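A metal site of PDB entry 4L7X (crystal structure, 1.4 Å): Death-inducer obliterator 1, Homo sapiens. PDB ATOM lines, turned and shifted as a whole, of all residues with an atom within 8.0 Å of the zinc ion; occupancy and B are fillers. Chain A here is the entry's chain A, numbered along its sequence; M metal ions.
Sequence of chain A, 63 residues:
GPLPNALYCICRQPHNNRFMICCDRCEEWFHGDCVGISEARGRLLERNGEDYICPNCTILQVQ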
ATOM      1  N   CYS A  22     -19.986  33.340 -10.385  1.00  0.00           N
ATOM      2  CA  CYS A  22     -19.926  31.890 -10.488  1.00  0.00           C
ATOM      3  C   CYS A  22     -18.739  31.471 -11.343  1.00  0.00           C
ATOM      4  O   CYS A  22     -18.464  32.085 -12.380  1.00  0.00           O
ATOM      5  CB  CYS A  22     -21.213  31.364 -11.114  1.00  0.00           C
ATOM      6  SG  CYS A  22     -21.445  29.575 -11.014  1.00  0.00           S
ATOM      7  N   CYS A  23     -18.043  30.433 -10.909  1.00  0.00           N
ATOM      8  CA  CYS A  23     -16.918  29.883 -11.668  1.00  0.00           C
ATOM      9  C   CYS A  23     -17.402  28.951 -12.759  1.00  0.00           C
ATOM     10  O   CYS A  23     -18.141  27.993 -12.501  1.00  0.00           O
ATOM     11  CB  CYS A  23     -15.976  29.110 -10.752  1.00  0.00           C
ATOM     12  SG  CYS A  23     -14.559  28.420 -11.650  1.00  0.00           S
ATOM     13  N   ASP A  24     -16.932  29.203 -13.979  1.00  0.00           N
ATOM     14  CA  ASP A  24     -17.351  28.415 -15.127  1.00  0.00           C
ATOM     15  C   ASP A  24     -16.612  27.079 -15.252  1.00  0.00           C
ATOM     16  O   ASP A  24     -16.947  26.267 -16.131  1.00  0.00           O
ATOM     17  CB  ASP A  24     -17.210  29.262 -16.389  1.00  0.00           C
ATOM     18  CG  ASP A  24     -18.242  30.359 -16.435  1.00  0.00           C
ATOM     19  OD1 ASP A  24     -19.416  30.019 -16.597  1.00  0.00           O
ATOM     20  OD2 ASP A  24     -17.891  31.564 -16.273  1.00  0.00           O
ATOM     21  N   ARG A  25     -15.633  26.848 -14.396  1.00  0.00           N
ATOM     22  CA  ARG A  25     -14.939  25.567 -14.355  1.00  0.00           C
ATOM     23  C   ARG A  25     -15.429  24.626 -13.256  1.00  0.00           C
ATOM     24  O   ARG A  25     -15.566  23.424 -13.496  1.00  0.00           O
ATOM     25  CB  ARG A  25     -13.431  25.769 -14.262  1.00  0.00           C
ATOM     26  CG  ARG A  25     -12.634  24.463 -14.280  1.00  0.00           C
ATOM     27  CZ  ARG A  25      -9.649  23.955 -13.080  1.00  0.00           C
ATOM     28  N   CYS A  26     -15.727  25.151 -12.067  1.00  0.00           N
ATOM     29  CA  CYS A  26     -16.183  24.291 -10.961  1.00  0.00           C
ATOM     30  C   CYS A  26     -17.633  24.518 -10.506  1.00  0.00           C
ATOM     31  O   CYS A  26     -18.140  23.759  -9.671  1.00  0.00           O
ATOM     32  CB  CYS A  26     -15.263  24.418  -9.746  1.00  0.00           C
ATOM     33  SG  CYS A  26     -15.380  26.014  -8.896  1.00  0.00           S
ATOM     34  N   GLU A  27     -18.268  25.572 -11.034  1.00  0.00           N
ATOM     35  CA  GLU A  27     -19.688  25.870 -10.774  1.00  0.00           C
ATOM     36  C   GLU A  27     -19.985  26.292  -9.336  1.00  0.00           C
ATOM     37  O   GLU A  27     -21.149  26.355  -8.937  1.00  0.00           O
ATOM     38  CB  GLU A  27     -20.577  24.700 -11.223  1.00  0.00           C
ATOM     39  CG  GLU A  27     -20.562  24.510 -12.733  1.00  0.00           C
ATOM     40  CD  GLU A  27     -21.283  25.626 -13.480  1.00  0.00           C
ATOM     41  OE1 GLU A  27     -22.321  26.111 -12.974  1.00  0.00           O
ATOM     42  OE2 GLU A  27     -20.836  26.005 -14.575  1.00  0.00           O
ATOM     43  N   GLU A  28     -18.940  26.572  -8.566  1.00  0.00           N
ATOM     44  CA  GLU A  28     -19.115  27.170  -7.239  1.00  0.00           C
ATOM     45  C   GLU A  28     -19.316  28.688  -7.390  1.00  0.00           C
ATOM     46  O   GLU A  28     -18.871  29.288  -8.370  1.00  0.00           O
ATOM     47  CB  GLU A  28     -17.903  26.854  -6.352  1.00  0.00           C
ATOM     48  CG  GLU A  28     -17.927  27.514  -4.968  1.00  0.00           C
ATOM     49  CD  GLU A  28     -19.031  27.008  -4.068  1.00  0.00           C
ATOM     50  OE1 GLU A  28     -20.180  27.516  -4.193  1.00  0.00           O
ATOM     51  OE2 GLU A  28     -18.775  26.092  -3.239  1.00  0.00           O
ATOM     52  N   TRP A  29     -20.027  29.274  -6.431  1.00  0.00           N
ATOM     53  CA  TRP A  29     -20.204  30.716  -6.351  1.00  0.00           C
ATOM     54  C   TRP A  29     -19.242  31.331  -5.343  1.00  0.00           C
ATOM     55  O   TRP A  29     -19.007  30.750  -4.268  1.00  0.00           O
ATOM     56  CB  TRP A  29     -21.632  31.063  -5.953  1.00  0.00           C
ATOM     57  CG  TRP A  29     -22.636  30.867  -7.031  1.00  0.00           C
ATOM     58  CD1 TRP A  29     -23.310  29.723  -7.339  1.00  0.00           C
ATOM     59  CD2 TRP A  29     -23.079  31.867  -7.960  1.00  0.00           C
ATOM     60  NE1 TRP A  29     -24.145  29.940  -8.397  1.00  0.00           N
ATOM     61  CE2 TRP A  29     -24.029  31.248  -8.796  1.00  0.00           C
ATOM     62  CE3 TRP A  29     -22.776  33.210  -8.158  1.00  0.00           C
ATOM     63  CZ2 TRP A  29     -24.679  31.939  -9.813  1.00  0.00           C
ATOM     64  CZ3 TRP A  29     -23.420  33.890  -9.182  1.00  0.00           C
ATOM     65  CH2 TRP A  29     -24.360  33.259  -9.980  1.00  0.00           C
ATOM     66  N   PHE A  30     -18.734  32.504  -5.678  1.00  0.00           N
ATOM     67  CA  PHE A  30     -17.705  33.184  -4.894  1.00  0.00           C
ATOM     68  C   PHE A  30     -18.121  34.628  -4.617  1.00  0.00           C
ATOM     69  O   PHE A  30     -18.602  35.317  -5.502  1.00  0.00           O
ATOM     70  CB  PHE A  30     -16.366  33.141  -5.636  1.00  0.00           C
ATOM     71  CG  PHE A  30     -15.862  31.749  -5.823  1.00  0.00           C
ATOM     72  CD1 PHE A  30     -16.245  31.014  -6.938  1.00  0.00           C
ATOM     73  CD2 PHE A  30     -15.058  31.151  -4.871  1.00  0.00           C
ATOM     74  CE1 PHE A  30     -15.809  29.703  -7.093  1.00  0.00           C
ATOM     75  CE2 PHE A  30     -14.636  29.839  -5.022  1.00  0.00           C
ATOM     76  CZ  PHE A  30     -15.014  29.128  -6.139  1.00  0.00           C
ATOM     77  N   TYR A  52     -15.606  33.194 -16.081  1.00  0.00           N
ATOM     78  CA  TYR A  52     -14.857  33.478 -14.870  1.00  0.00           C
ATOM     79  C   TYR A  52     -14.257  32.176 -14.354  1.00  0.00           C
ATOM     80  O   TYR A  52     -14.958  31.158 -14.236  1.00  0.00           O
ATOM     81  CB  TYR A  52     -15.741  34.126 -13.783  1.00  0.00           C
ATOM     82  CG  TYR A  52     -14.972  34.231 -12.506  1.00  0.00           C
ATOM     83  CD1 TYR A  52     -13.896  35.103 -12.388  1.00  0.00           C
ATOM     84  CD2 TYR A  52     -15.260  33.405 -11.425  1.00  0.00           C
ATOM     85  CE1 TYR A  52     -13.157  35.179 -11.227  1.00  0.00           C
ATOM     86  CE2 TYR A  52     -14.533  33.485 -10.252  1.00  0.00           C
ATOM     87  CZ  TYR A  52     -13.466  34.356 -10.166  1.00  0.00           C
ATOM     88  OH  TYR A  52     -12.721  34.422  -9.013  1.00  0.00           O
ATOM     89  N   ILE A  53     -12.968  32.208 -14.048  1.00  0.00           N
ATOM     90  CA  ILE A  53     -12.241  31.064 -13.497  1.00  0.00           C
ATOM     91  C   ILE A  53     -11.718  31.447 -12.107  1.00  0.00           C
ATOM     92  O   ILE A  53     -10.941  32.413 -11.962  1.00  0.00           O
ATOM     93  CB  ILE A  53     -11.073  30.647 -14.394  1.00  0.00           C
ATOM     94  CG1 ILE A  53     -11.569  30.393 -15.824  1.00  0.00           C
ATOM     95  CG2 ILE A  53     -10.370  29.420 -13.840  1.00  0.00           C
ATOM     96  CD1 ILE A  53     -12.674  29.380 -15.942  1.00  0.00           C
ATOM     97  N   CYS A  54     -12.179  30.714 -11.100  1.00  0.00           N
ATOM     98  CA  CYS A  54     -11.903  31.054  -9.706  1.00  0.00           C
ATOM     99  C   CYS A  54     -10.460  30.698  -9.341  1.00  0.00           C
ATOM    100  O   CYS A  54      -9.764  30.011 -10.106  1.00  0.00           O
ATOM    101  CB  CYS A  54     -12.863  30.311  -8.776  1.00  0.00           C
ATOM    102  SG  CYS A  54     -12.408  28.579  -8.439  1.00  0.00           S
ATOM    103  N   PRO A  55     -10.014  31.126  -8.163  1.00  0.00           N
ATOM    104  CA  PRO A  55      -8.641  30.838  -7.746  1.00  0.00           C
ATOM    105  C   PRO A  55      -8.343  29.356  -7.558  1.00  0.00           C
ATOM    106  O   PRO A  55      -7.221  28.920  -7.856  1.00  0.00           O
ATOM    107  CB  PRO A  55      -8.511  31.608  -6.425  1.00  0.00           C
ATOM    108  CG  PRO A  55      -9.514  32.713  -6.551  1.00  0.00           C
ATOM    109  CD  PRO A  55     -10.667  32.097  -7.268  1.00  0.00           C
ATOM    110  N   ASN A  56      -9.304  28.564  -7.065  1.00  0.00           N
ATOM    111  CA  ASN A  56      -9.071  27.132  -6.862  1.00  0.00           C
ATOM    112  C   ASN A  56      -8.788  26.491  -8.206  1.00  0.00           C
ATOM    113  O   ASN A  56      -8.003  25.552  -8.330  1.00  0.00           O
ATOM    114  CB  ASN A  56     -10.285  26.409  -6.261  1.00  0.00           C
ATOM    115  CG  ASN A  56     -10.671  26.917  -4.891  1.00  0.00           C
ATOM    116  OD1 ASN A  56      -9.830  27.345  -4.113  1.00  0.00           O
ATOM    117  ND2 ASN A  56     -11.967  26.822  -4.573  1.00  0.00           N
ATOM    118  N   CYS A  57      -9.490  26.998  -9.206  1.00  0.00           N
ATOM    119  CA  CYS A  57      -9.446  26.427 -10.525  1.00  0.00           C
ATOM    120  C   CYS A  57      -8.306  26.969 -11.396  1.00  0.00           C
ATOM    121  O   CYS A  57      -8.086  26.485 -12.516  1.00  0.00           O
ATOM    122  CB  CYS A  57     -10.783  26.674 -11.242  1.00  0.00           C
ATOM    123  SG  CYS A  57     -12.089  25.587 -10.669  1.00  0.00           S
ATOM    124  N   THR A  58      -7.589  27.968 -10.907  1.00  0.00           N
ATOM    125  CA  THR A  58      -6.416  28.452 -11.593  1.00  0.00           C
ATOM    126  C   THR A  58      -5.213  27.578 -11.210  1.00  0.00           C
ATOM    127  O   THR A  58      -4.939  27.390 -10.025  1.00  0.00           O
ATOM    128  CB  THR A  58      -6.091  29.881 -11.218  1.00  0.00           C
ATOM    129  CG2 THR A  58      -7.330  30.720 -11.343  1.00  0.00           C
HETATM  130 ZN    ZN M   1     -13.610  27.173  -9.899  1.00  0.00          ZN
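The side-chain sulfur (SG) of Cys 23 lies close to the backbone carbonyl oxygen (O) of Tyr 52, 3.8 Å away.
The side-chain sulfur (SG) of Cys 23 lies close to the backbone NH (N) of Arg 25 (3.3 Å).
The side-chain sulfur of Cys 26 lies close to the backbone NH of Glu 28.
The backbone carbonyl oxygen (O) of Glu 28 sits at hydrogen-bond distance from the backbone NH (N) of Cys 23 (2.9 Å).
SG of Cys 54 sits close to N of Asn 56, 3.4 Å away.
Of the 16 residues printed, 4 come within 4 Å of the zinc ion.
The zinc ion is bound by the side-chain sulfur (SG) of Cys 57.
SG of Cys 26 binds the zinc ion (2.3 Å).
The side-chain sulfur (SG) of Cys 23 binds the zinc ion (2.3 Å).
SG of Cys 54 binds the zinc ion, 2.4 Å away.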
